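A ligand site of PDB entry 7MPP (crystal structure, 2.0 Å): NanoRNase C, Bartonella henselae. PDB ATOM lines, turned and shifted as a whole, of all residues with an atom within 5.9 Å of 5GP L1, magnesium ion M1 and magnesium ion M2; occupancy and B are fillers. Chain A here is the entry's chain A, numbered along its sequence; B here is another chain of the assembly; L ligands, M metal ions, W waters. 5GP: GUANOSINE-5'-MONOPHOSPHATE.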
ATOM      1  N   ASP A  26       4.375  16.987   8.551  1.00  0.00           N
ATOM      2  CA  ASP A  26       5.363  15.910   8.614  1.00  0.00           C
ATOM      3  C   ASP A  26       5.611  15.600  10.084  1.00  0.00           C
ATOM      4  O   ASP A  26       5.217  16.368  10.981  1.00  0.00           O
ATOM      5  CB  ASP A  26       6.659  16.305   7.896  1.00  0.00           C
ATOM      6  CG  ASP A  26       7.660  15.157   7.804  1.00  0.00           C
ATOM      7  OD1 ASP A  26       7.246  14.023   7.545  1.00  0.00           O
ATOM      8  OD2 ASP A  26       8.869  15.398   8.007  1.00  0.00           O
ATOM      9  N   THR A  27       6.241  14.459  10.348  1.00  0.00           N
ATOM     10  CA  THR A  27       6.568  14.065  11.719  1.00  0.00           C
ATOM     11  C   THR A  27       7.986  13.503  11.780  1.00  0.00           C
ATOM     12  O   THR A  27       8.512  12.990  10.791  1.00  0.00           O
ATOM     13  CB  THR A  27       5.592  13.021  12.290  1.00  0.00           C
ATOM     14  OG1 THR A  27       5.681  11.799  11.529  1.00  0.00           O
ATOM     15  CG2 THR A  27       4.162  13.521  12.234  1.00  0.00           C
ATOM     16  N   GLU A  28       8.579  13.584  12.969  1.00  0.00           N
ATOM     17  CA  GLU A  28       9.774  12.827  13.312  1.00  0.00           C
ATOM     18  C   GLU A  28       9.483  11.961  14.528  1.00  0.00           C
ATOM     19  O   GLU A  28       8.752  12.380  15.431  1.00  0.00           O
ATOM     20  CB  GLU A  28      10.966  13.749  13.590  1.00  0.00           C
ATOM     21  CG  GLU A  28      11.156  14.818  12.552  1.00  0.00           C
ATOM     22  CD  GLU A  28      11.560  14.245  11.217  1.00  0.00           C
ATOM     23  OE1 GLU A  28      12.085  13.104  11.184  1.00  0.00           O
ATOM     24  OE2 GLU A  28      11.352  14.942  10.202  1.00  0.00           O
ATOM     25  N   THR A  29      10.070  10.776  14.552  1.00  0.00           N
ATOM     26  CA  THR A  29       9.778   9.764  15.559  1.00  0.00           C
ATOM     27  C   THR A  29      11.076   9.053  15.935  1.00  0.00           C
ATOM     28  O   THR A  29      12.136   9.301  15.343  1.00  0.00           O
ATOM     29  CB  THR A  29       8.812   8.703  15.026  1.00  0.00           C
ATOM     30  OG1 THR A  29       9.487   7.978  14.013  1.00  0.00           O
ATOM     31  CG2 THR A  29       7.523   9.308  14.448  1.00  0.00           C
ATOM     32  N   LEU A  30      10.981   8.110  16.869  1.00  0.00           N
ATOM     33  CA  LEU A  30      12.111   7.250  17.175  1.00  0.00           C
ATOM     34  C   LEU A  30      12.190   6.038  16.242  1.00  0.00           C
ATOM     35  O   LEU A  30      13.007   5.158  16.468  1.00  0.00           O
ATOM     36  CB  LEU A  30      12.060   6.777  18.637  1.00  0.00           C
ATOM     37  CG  LEU A  30      12.538   7.825  19.641  1.00  0.00           C
ATOM     38  CD1 LEU A  30      12.300   7.364  21.080  1.00  0.00           C
ATOM     39  CD2 LEU A  30      14.027   8.108  19.417  1.00  0.00           C
ATOM     40  N   GLY A  31      11.378   5.985  15.206  1.00  0.00           N
ATOM     41  CA  GLY A  31      11.460   4.897  14.253  1.00  0.00           C
ATOM     42  C   GLY A  31      10.129   4.669  13.558  1.00  0.00           C
ATOM     43  O   GLY A  31       9.204   5.464  13.663  1.00  0.00           O
ATOM     44  N   LEU A  32      10.052   3.533  12.860  1.00  0.00           N
ATOM     45  CA  LEU A  32       8.952   3.279  11.931  1.00  0.00           C
ATOM     46  C   LEU A  32       7.814   2.466  12.533  1.00  0.00           C
ATOM     47  O   LEU A  32       6.858   2.163  11.819  1.00  0.00           O
ATOM     48  CB  LEU A  32       9.467   2.555  10.697  1.00  0.00           C
ATOM     49  CG  LEU A  32      10.542   3.327   9.933  1.00  0.00           C
ATOM     50  CD1 LEU A  32      11.085   2.488   8.801  1.00  0.00           C
ATOM     51  CD2 LEU A  32       9.970   4.621   9.409  1.00  0.00           C
ATOM     52  N   GLN A  43       5.754  18.803  12.360  1.00  0.00           N
ATOM     53  CA  GLN A  43       6.115  20.018  11.653  1.00  0.00           C
ATOM     54  C   GLN A  43       4.941  20.443  10.786  1.00  0.00           C
ATOM     55  O   GLN A  43       4.239  19.598  10.223  1.00  0.00           O
ATOM     56  CB  GLN A  43       7.348  19.821  10.777  1.00  0.00           C
ATOM     57  CG  GLN A  43       8.544  19.264  11.506  1.00  0.00           C
ATOM     58  CD  GLN A  43       8.665  17.750  11.354  1.00  0.00           C
ATOM     59  OE1 GLN A  43       8.339  17.007  12.266  1.00  0.00           O
ATOM     60  NE2 GLN A  43       9.148  17.312  10.195  1.00  0.00           N
ATOM     61  N   HIS A  80       4.209  13.918   2.543  1.00  0.00           N
ATOM     62  CA  HIS A  80       4.937  13.006   1.659  1.00  0.00           C
ATOM     63  C   HIS A  80       4.967  11.635   2.314  1.00  0.00           C
ATOM     64  O   HIS A  80       5.616  11.459   3.348  1.00  0.00           O
ATOM     65  CB  HIS A  80       6.355  13.476   1.355  1.00  0.00           C
ATOM     66  CG  HIS A  80       7.081  12.520   0.466  1.00  0.00           C
ATOM     67  ND1 HIS A  80       6.913  12.501  -0.902  1.00  0.00           N
ATOM     68  CD2 HIS A  80       7.926  11.499   0.755  1.00  0.00           C
ATOM     69  CE1 HIS A  80       7.643  11.523  -1.417  1.00  0.00           C
ATOM     70  NE2 HIS A  80       8.270  10.909  -0.431  1.00  0.00           N
ATOM     71  N   PHE A  81       4.301  10.676   1.683  1.00  0.00           N
ATOM     72  CA  PHE A  81       4.070   9.333   2.227  1.00  0.00           C
ATOM     73  C   PHE A  81       3.325   9.444   3.556  1.00  0.00           C
ATOM     74  O   PHE A  81       3.827   9.053   4.616  1.00  0.00           O
ATOM     75  CB  PHE A  81       5.372   8.541   2.379  1.00  0.00           C
ATOM     76  CG  PHE A  81       5.148   7.043   2.594  1.00  0.00           C
ATOM     77  CD1 PHE A  81       4.395   6.306   1.698  1.00  0.00           C
ATOM     78  CD2 PHE A  81       5.716   6.386   3.691  1.00  0.00           C
ATOM     79  CE1 PHE A  81       4.183   4.926   1.895  1.00  0.00           C
ATOM     80  CE2 PHE A  81       5.509   5.016   3.888  1.00  0.00           C
ATOM     81  CZ  PHE A  81       4.748   4.282   2.980  1.00  0.00           C
ATOM     82  N   PHE A  84       2.532   6.811   6.629  1.00  0.00           N
ATOM     83  CA  PHE A  84       3.265   6.724   7.882  1.00  0.00           C
ATOM     84  C   PHE A  84       2.782   7.765   8.882  1.00  0.00           C
ATOM     85  O   PHE A  84       2.455   7.435  10.023  1.00  0.00           O
ATOM     86  CB  PHE A  84       4.766   6.885   7.649  1.00  0.00           C
ATOM     87  CG  PHE A  84       5.517   6.960   8.930  1.00  0.00           C
ATOM     88  CD1 PHE A  84       5.658   5.830   9.704  1.00  0.00           C
ATOM     89  CD2 PHE A  84       5.973   8.172   9.417  1.00  0.00           C
ATOM     90  CE1 PHE A  84       6.309   5.880  10.941  1.00  0.00           C
ATOM     91  CE2 PHE A  84       6.625   8.243  10.642  1.00  0.00           C
ATOM     92  CZ  PHE A  84       6.788   7.090  11.409  1.00  0.00           C
ATOM     93  N   ASP A  85       2.774   9.042   8.478  1.00  0.00           N
ATOM     94  CA  ASP A  85       2.455  10.115   9.416  1.00  0.00           C
ATOM     95  C   ASP A  85       1.037   9.976   9.934  1.00  0.00           C
ATOM     96  O   ASP A  85       0.764  10.238  11.112  1.00  0.00           O
ATOM     97  CB  ASP A  85       2.636  11.469   8.746  1.00  0.00           C
ATOM     98  CG  ASP A  85       4.037  11.664   8.242  1.00  0.00           C
ATOM     99  OD1 ASP A  85       4.959  11.831   9.085  1.00  0.00           O
ATOM    100  OD2 ASP A  85       4.222  11.622   7.011  1.00  0.00           O
ATOM    101  N   LYS A 133      19.146  14.474   3.708  1.00  0.00           N
ATOM    102  CA  LYS A 133      18.583  13.497   4.633  1.00  0.00           C
ATOM    103  C   LYS A 133      19.539  13.128   5.763  1.00  0.00           C
ATOM    104  O   LYS A 133      19.311  12.124   6.451  1.00  0.00           O
ATOM    105  CB  LYS A 133      18.139  12.234   3.890  1.00  0.00           C
ATOM    106  CG  LYS A 133      17.151  12.459   2.729  1.00  0.00           C
ATOM    107  CD  LYS A 133      16.046  13.494   3.074  1.00  0.00           C
ATOM    108  CE  LYS A 133      14.936  12.930   3.959  1.00  0.00           C
ATOM    109  NZ  LYS A 133      13.915  13.967   4.390  1.00  0.00           N
ATOM    110  N   GLN A 136      17.976  12.746   9.227  1.00  0.00           N
ATOM    111  CA  GLN A 136      16.879  11.786   9.351  1.00  0.00           C
ATOM    112  C   GLN A 136      17.168  10.782  10.456  1.00  0.00           C
ATOM    113  O   GLN A 136      16.344  10.586  11.361  1.00  0.00           O
ATOM    114  CB  GLN A 136      16.671  11.088   8.005  1.00  0.00           C
ATOM    115  CG  GLN A 136      15.597  10.017   7.978  1.00  0.00           C
ATOM    116  CD  GLN A 136      15.459   9.394   6.601  1.00  0.00           C
ATOM    117  OE1 GLN A 136      14.480   9.644   5.892  1.00  0.00           O
ATOM    118  NE2 GLN A 136      16.454   8.604   6.199  1.00  0.00           N
ATOM    119  N   SER A 137      18.338  10.150  10.425  1.00  0.00           N
ATOM    120  CA  SER A 137      18.724   9.202  11.462  1.00  0.00           C
ATOM    121  C   SER A 137      19.466   9.977  12.546  1.00  0.00           C
ATOM    122  O   SER A 137      20.687  10.167  12.493  1.00  0.00           O
ATOM    123  CB  SER A 137      19.559   8.070  10.885  1.00  0.00           C
ATOM    124  OG  SER A 137      18.767   7.286  10.000  1.00  0.00           O
ATOM    125  N   SER A 138      18.713  10.435  13.534  1.00  0.00           N
ATOM    126  CA  SER A 138      19.240  11.184  14.656  1.00  0.00           C
ATOM    127  C   SER A 138      18.286  10.992  15.814  1.00  0.00           C
ATOM    128  O   SER A 138      17.173  10.478  15.639  1.00  0.00           O
ATOM    129  CB  SER A 138      19.412  12.672  14.327  1.00  0.00           C
ATOM    130  OG  SER A 138      18.156  13.323  14.200  1.00  0.00           O
ATOM    131  N   TRP A 140      15.671  11.923  17.674  1.00  0.00           N
ATOM    132  CA  TRP A 140      14.582  12.885  17.614  1.00  0.00           C
ATOM    133  C   TRP A 140      13.891  13.093  18.958  1.00  0.00           C
ATOM    134  O   TRP A 140      13.116  14.057  19.090  1.00  0.00           O
ATOM    135  CB  TRP A 140      13.591  12.449  16.546  1.00  0.00           C
ATOM    136  CG  TRP A 140      14.143  12.723  15.174  1.00  0.00           C
ATOM    137  CD1 TRP A 140      14.580  11.802  14.262  1.00  0.00           C
ATOM    138  CD2 TRP A 140      14.334  14.005  14.571  1.00  0.00           C
ATOM    139  NE1 TRP A 140      15.029  12.432  13.125  1.00  0.00           N
ATOM    140  CE2 TRP A 140      14.885  13.787  13.299  1.00  0.00           C
ATOM    141  CE3 TRP A 140      14.094  15.322  15.002  1.00  0.00           C
ATOM    142  CZ2 TRP A 140      15.192  14.832  12.431  1.00  0.00           C
ATOM    143  CZ3 TRP A 140      14.404  16.353  14.136  1.00  0.00           C
ATOM    144  CH2 TRP A 140      14.949  16.104  12.866  1.00  0.00           C
ATOM    145  N   TYR A 152      16.295  20.505   9.235  1.00  0.00           N
ATOM    146  CA  TYR A 152      15.847  19.336   8.484  1.00  0.00           C
ATOM    147  C   TYR A 152      14.353  19.133   8.641  1.00  0.00           C
ATOM    148  O   TYR A 152      13.629  18.939   7.652  1.00  0.00           O
ATOM    149  CB  TYR A 152      16.605  18.096   8.957  1.00  0.00           C
ATOM    150  CG  TYR A 152      15.988  16.803   8.476  1.00  0.00           C
ATOM    151  CD1 TYR A 152      16.324  16.273   7.244  1.00  0.00           C
ATOM    152  CD2 TYR A 152      15.059  16.110   9.263  1.00  0.00           C
ATOM    153  CE1 TYR A 152      15.759  15.078   6.789  1.00  0.00           C
ATOM    154  CE2 TYR A 152      14.493  14.917   8.828  1.00  0.00           C
ATOM    155  CZ  TYR A 152      14.853  14.407   7.586  1.00  0.00           C
ATOM    156  OH  TYR A 152      14.297  13.231   7.140  1.00  0.00           O
ATOM    157  N   ALA A 153      13.875  19.146   9.884  1.00  0.00           N
ATOM    158  CA  ALA A 153      12.447  18.932  10.117  1.00  0.00           C
ATOM    159  C   ALA A 153      11.609  19.952   9.355  1.00  0.00           C
ATOM    160  O   ALA A 153      10.604  19.599   8.722  1.00  0.00           O
ATOM    161  CB  ALA A 153      12.172  18.990  11.622  1.00  0.00           C
ATOM    162  N   ASP A 156      11.310  19.498   5.440  1.00  0.00           N
ATOM    163  CA  ASP A 156      10.410  18.448   4.991  1.00  0.00           C
ATOM    164  C   ASP A 156       8.981  18.942   4.794  1.00  0.00           C
ATOM    165  O   ASP A 156       8.202  18.230   4.155  1.00  0.00           O
ATOM    166  CB  ASP A 156      10.426  17.283   5.980  1.00  0.00           C
ATOM    167  CG  ASP A 156      11.499  16.233   5.634  1.00  0.00           C
ATOM    168  OD1 ASP A 156      12.266  16.482   4.681  1.00  0.00           O
ATOM    169  OD2 ASP A 156      11.566  15.175   6.307  1.00  0.00           O
ATOM    170  N   ARG B 111      18.706   2.786  18.823  1.00  0.00           N
ATOM    171  CA  ARG B 111      18.733   3.547  17.577  1.00  0.00           C
ATOM    172  C   ARG B 111      17.752   2.936  16.575  1.00  0.00           C
ATOM    173  O   ARG B 111      18.096   2.453  15.501  1.00  0.00           O
ATOM    174  CB  ARG B 111      20.154   3.626  17.034  1.00  0.00           C
ATOM    175  CG  ARG B 111      21.054   4.432  17.995  1.00  0.00           C
ATOM    176  CD  ARG B 111      22.515   4.424  17.581  1.00  0.00           C
ATOM    177  NE  ARG B 111      22.720   5.083  16.296  1.00  0.00           N
ATOM    178  CZ  ARG B 111      22.982   4.460  15.157  1.00  0.00           C
ATOM    179  NH1 ARG B 111      23.067   3.133  15.128  1.00  0.00           N
ATOM    180  NH2 ARG B 111      23.153   5.157  14.057  1.00  0.00           N
ATOM    181  N   THR B 112      16.485   2.982  16.988  1.00  0.00           N
ATOM    182  CA  THR B 112      15.398   2.394  16.218  1.00  0.00           C
ATOM    183  C   THR B 112      15.042   3.236  15.000  1.00  0.00           C
ATOM    184  O   THR B 112      14.263   2.792  14.159  1.00  0.00           O
ATOM    185  CB  THR B 112      14.178   2.194  17.137  1.00  0.00           C
ATOM    186  OG1 THR B 112      13.998   3.366  17.946  1.00  0.00           O
ATOM    187  CG2 THR B 112      14.421   1.013  18.083  1.00  0.00           C
ATOM    188  N   TYR B 113      15.601   4.434  14.912  1.00  0.00           N
ATOM    189  CA  TYR B 113      15.383   5.340  13.799  1.00  0.00           C
ATOM    190  C   TYR B 113      16.352   5.110  12.646  1.00  0.00           C
ATOM    191  O   TYR B 113      16.439   5.944  11.750  1.00  0.00           O
ATOM    192  CB  TYR B 113      15.490   6.774  14.294  1.00  0.00           C
ATOM    193  CG  TYR B 113      16.691   7.038  15.199  1.00  0.00           C
ATOM    194  CD1 TYR B 113      17.974   7.185  14.680  1.00  0.00           C
ATOM    195  CD2 TYR B 113      16.523   7.180  16.574  1.00  0.00           C
ATOM    196  CE1 TYR B 113      19.076   7.445  15.518  1.00  0.00           C
ATOM    197  CE2 TYR B 113      17.595   7.445  17.399  1.00  0.00           C
ATOM    198  CZ  TYR B 113      18.869   7.573  16.871  1.00  0.00           C
ATOM    199  OH  TYR B 113      19.926   7.837  17.716  1.00  0.00           O
ATOM    200  N   THR B 114      17.113   4.011  12.685  1.00  0.00           N
ATOM    201  CA  THR B 114      18.034   3.673  11.618  1.00  0.00           C
ATOM    202  C   THR B 114      18.136   2.161  11.545  1.00  0.00           C
ATOM    203  O   THR B 114      17.721   1.446  12.469  1.00  0.00           O
ATOM    204  CB  THR B 114      19.431   4.268  11.825  1.00  0.00           C
ATOM    205  OG1 THR B 114      20.277   3.891  10.726  1.00  0.00           O
ATOM    206  CG2 THR B 114      20.065   3.708  13.120  1.00  0.00           C
ATOM    207  N   ASP B 115      18.702   1.679  10.456  1.00  0.00           N
ATOM    208  CA  ASP B 115      19.000   0.271  10.287  1.00  0.00           C
ATOM    209  C   ASP B 115      20.500   0.014  10.228  1.00  0.00           C
ATOM    210  O   ASP B 115      20.923  -1.133  10.047  1.00  0.00           O
ATOM    211  CB  ASP B 115      18.297  -0.246   9.024  1.00  0.00           C
ATOM    212  CG  ASP B 115      16.892   0.339   8.862  1.00  0.00           C
ATOM    213  OD1 ASP B 115      16.106   0.286   9.839  1.00  0.00           O
ATOM    214  OD2 ASP B 115      16.574   0.889   7.781  1.00  0.00           O
HETATM  215  P   5GP L   1      11.378  11.632   7.946  1.00  0.00           P
HETATM  216  O1P 5GP L   1      12.409  12.392   8.739  1.00  0.00           O
HETATM  217  O2P 5GP L   1      10.018  12.310   7.850  1.00  0.00           O
HETATM  218  O3P 5GP L   1      11.937  11.190   6.611  1.00  0.00           O
HETATM  219  O5' 5GP L   1      11.191  10.252   8.738  1.00  0.00           O
HETATM  220  C5' 5GP L   1      10.302  10.126   9.854  1.00  0.00           C
HETATM  221  C4' 5GP L   1      10.881   9.219  10.921  1.00  0.00           C
HETATM  222  O4' 5GP L   1      11.015   7.878  10.394  1.00  0.00           O
HETATM  223  C3' 5GP L   1      12.275   9.597  11.397  1.00  0.00           C
HETATM  224  O3' 5GP L   1      12.228  10.543  12.454  1.00  0.00           O
HETATM  225  C2' 5GP L   1      12.918   8.258  11.789  1.00  0.00           C
HETATM  226  O2' 5GP L   1      12.613   7.924  13.133  1.00  0.00           O
HETATM  227  C1' 5GP L   1      12.179   7.260  10.895  1.00  0.00           C
HETATM  228  N9  5GP L   1      12.987   6.787   9.750  1.00  0.00           N
HETATM  229  C8  5GP L   1      13.183   7.409   8.567  1.00  0.00           C
HETATM  230  N7  5GP L   1      13.919   6.611   7.766  1.00  0.00           N
HETATM  231  C5  5GP L   1      14.161   5.454   8.428  1.00  0.00           C
HETATM  232  C6  5GP L   1      14.843   4.271   8.127  1.00  0.00           C
HETATM  233  O6  5GP L   1      15.403   4.102   7.022  1.00  0.00           O
HETATM  234  N1  5GP L   1      14.882   3.297   9.042  1.00  0.00           N
HETATM  235  C2  5GP L   1      14.292   3.429  10.239  1.00  0.00           C
HETATM  236  N2  5GP L   1      14.353   2.431  11.147  1.00  0.00           N
HETATM  237  N3  5GP L   1      13.624   4.559  10.555  1.00  0.00           N
HETATM  238  C4  5GP L   1      13.549   5.577   9.664  1.00  0.00           C
HETATM  239  P   5GP L   2      11.058   8.633   0.694  1.00  0.00           P
HETATM  240  O1P 5GP L   2      12.154   7.788   0.052  1.00  0.00           O
HETATM  241  O2P 5GP L   2      11.374  10.098   0.930  1.00  0.00           O
HETATM  242  O3P 5GP L   2       9.709   8.464   0.053  1.00  0.00           O
HETATM  243  O5' 5GP L   2      10.879   7.966   2.123  1.00  0.00           O
HETATM  244  C5' 5GP L   2       9.821   8.351   2.996  1.00  0.00           C
HETATM  245  C4' 5GP L   2      10.122   7.963   4.415  1.00  0.00           C
HETATM  246  O4' 5GP L   2      10.036   6.510   4.566  1.00  0.00           O
HETATM  247  C3' 5GP L   2      11.512   8.355   4.900  1.00  0.00           C
HETATM  248  O3' 5GP L   2      11.464   8.671   6.289  1.00  0.00           O
HETATM  249  C2' 5GP L   2      12.308   7.065   4.685  1.00  0.00           C
HETATM  250  O2' 5GP L   2      13.491   6.941   5.438  1.00  0.00           O
HETATM  251  C1' 5GP L   2      11.269   6.014   5.061  1.00  0.00           C
HETATM  252  N9  5GP L   2      11.514   4.709   4.448  1.00  0.00           N
HETATM  253  C8  5GP L   2      12.634   4.412   3.764  1.00  0.00           C
HETATM  254  N7  5GP L   2      12.555   3.138   3.317  1.00  0.00           N
HETATM  255  C5  5GP L   2      11.373   2.642   3.750  1.00  0.00           C
HETATM  256  C6  5GP L   2      10.776   1.409   3.587  1.00  0.00           C
HETATM  257  O6  5GP L   2      11.352   0.502   2.945  1.00  0.00           O
HETATM  258  N1  5GP L   2       9.569   1.198   4.136  1.00  0.00           N
HETATM  259  C2  5GP L   2       8.938   2.160   4.821  1.00  0.00           C
HETATM  260  N2  5GP L   2       7.715   1.876   5.344  1.00  0.00           N
HETATM  261  N3  5GP L   2       9.502   3.378   4.992  1.00  0.00           N
HETATM  262  C4  5GP L   2      10.719   3.631   4.461  1.00  0.00           C
HETATM  263 MG    MG M   1       8.212  12.225   6.870  1.00  0.00          MG
HETATM  264 MG    MG M   2      10.879  14.517   8.183  1.00  0.00          MG
HETATM  265  O   HOH W   1       6.337  12.090   5.940  1.00  0.00           O
HETATM  266  O   HOH W   2       8.872  10.176   6.214  1.00  0.00           O
HETATM  267  O   HOH W   3       7.558  11.502   8.744  1.00  0.00           O
HETATM  268  O   HOH W   4       8.957  13.316   5.103  1.00  0.00           O
HETATM  269  O   HOH W   5      11.375  12.050   4.131  1.00  0.00           O
HETATM  270  O   HOH W   6       9.423   7.849   7.594  1.00  0.00           O
HETATM  271  O   HOH W   7      12.079   1.648  12.977  1.00  0.00           O
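OH of Tyr 152 sits at hydrogen-bond distance from O1P of 5GP L1, at 2.6 Å. N of Thr 29 sits at hydrogen-bond distance from O3' of 5GP L1 (3.0 Å). The backbone carbonyl oxygen (O) of Thr 29 sits at hydrogen-bond distance from an oxygen (O2') of 5GP L1, at 2.6 Å. O2' of 5GP L1 sits at hydrogen-bond distance from OG1 of Thr 29 (3.2 Å). A nitrogen (N2) of 5GP L1 sits at hydrogen-bond distance from the backbone carbonyl oxygen of Thr 112 of chain B (3.0 Å). OE1 of Gln 136 lies close to O3P of 5GP L1 (3.1 Å). The side-chain carboxylate of Asp 115 of chain B is in hydrogen-bond range of a nitrogen (N2) of 5GP L1. The backbone NH of Gly 31 sits at hydrogen-bond distance from an oxygen (O2') of 5GP L1, 3.1 Å away. O3' of 5GP L1 lies close to NE1 of Trp 140 (3.4 Å). The side-chain amide oxygen (OE1) of Gln 136 sits at hydrogen-bond distance from an oxygen (O2') of 5GP L2 (2.9 Å). An oxygen (O3P) of 5GP L2 sits at hydrogen-bond distance from a ring nitrogen (NE2) of His 80 (2.9 Å).
An oxygen (O3P) of 5GP L1 is in hydrogen-bond range of an oxygen (O3') of 5GP L2.
The side-chain hydroxyl (OH) of Tyr 152 lies close to the side-chain carboxylate (OD2) of Asp 156 (3.5 Å). The side-chain amide nitrogen (NE2) of Gln 43 lies close to the side-chain carboxylate (OE2) of Glu 28, at 3.2 Å. OG1 of Thr 112 of chain B is in hydrogen-bond range of O of Leu 30, 2.5 Å away. NE1 of Trp 140 lies within hydrogen-bond range of O of Gln 136 (2.9 Å). The indole nitrogen (NE1) of Trp 140 lies close to the side-chain hydroxyl (OG) of Ser 138, 3.4 Å away. The backbone carbonyl oxygen of Leu 30 is in hydrogen-bond range of the backbone NH of Tyr 113 of chain B, at 3.1 Å. O of Tyr 113 of chain B lies within hydrogen-bond range of OG of Ser 137, 3.2 Å away. OG1 of Thr 27 sits at hydrogen-bond distance from OD1 of Asp 85.
The backbone carbonyl oxygen of Thr 27 lies close to an oxygen (O2P) of 5GP L1. The backbone carbonyl oxygen (O) of Tyr 113 of chain B lies close to a nitrogen (N3) of 5GP L1, at 3.4 Å. Merely in contact with 5GP L1: Leu 32, Thr 114 of chain B and Leu 30. Hydrophobic or aromatic side chains that line 5GP L1: Leu 32, Trp 140, Tyr 152 and Tyr 113 of chain B.
Residues that only touch magnesium ion M1: Asp 85 (3.96 Å). Of the 25 residues printed, 2 come within 4 Å of magnesium ion M1.
O of Thr 27 touches magnesium ion M2, 3.8 Å away. Gln 43 touches magnesium ion M2 (NE2 to MG, 3.9 Å). Tyr 152 touches magnesium ion M2 (CE2 to MG, 3.7 Å). Within 4 Å of magnesium ion M2: Asp 26, Thr 27, Glu 28, Gln 43, Tyr 152 and Asp 156. The nearest printed residue that does not touch magnesium ion M2 is Lys 133 (4.9 Å).
Magnesium ion M1 is bound by O2P of 5GP L1, at 2.1 Å. Water W1 is bound to magnesium ion M1. Water W3 binds magnesium ion M1, at 2.1 Å. OD1 of Asp 26 binds magnesium ion M1. Magnesium ion M1 is bound by water W4 (2.2 Å). Water W2 binds magnesium ion M1.
Magnesium ion M2 is bound by OD2 of Asp 156 (2.1 Å), OE2 of Glu 28 (2.1 Å), OD2 of Asp 26 (2.2 Å) and O2P of 5GP L1 (2.4 Å). Slightly farther from magnesium ion M2 lies O1P of 5GP L1 (2.7 Å).
Water W1 bridges OD2 of Asp 85 (2.4 Å) and O of His 80 (2.8 Å). Water W2 lies within hydrogen-bond range of an oxygen (O3') of 5GP L2 (3.0 Å) and an oxygen (O3P) of 5GP L1 (3.3 Å). Water W3 bridges OD1 of Asp 85 (2.6 Å) and O of Thr 27 (2.7 Å). Water W5 bridges an oxygen (O3P) of 5GP L1 (2.7 Å) and the side-chain amino group of Lys 133 (3.2 Å). Water W7 lies within hydrogen-bond range of O of Thr 112 of chain B (2.7 Å), N of Leu 32 (2.8 Å) and N2 of 5GP L1 (3.0 Å). Water W6 bridges O3' of 5GP L2 and O5' of 5GP L1.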
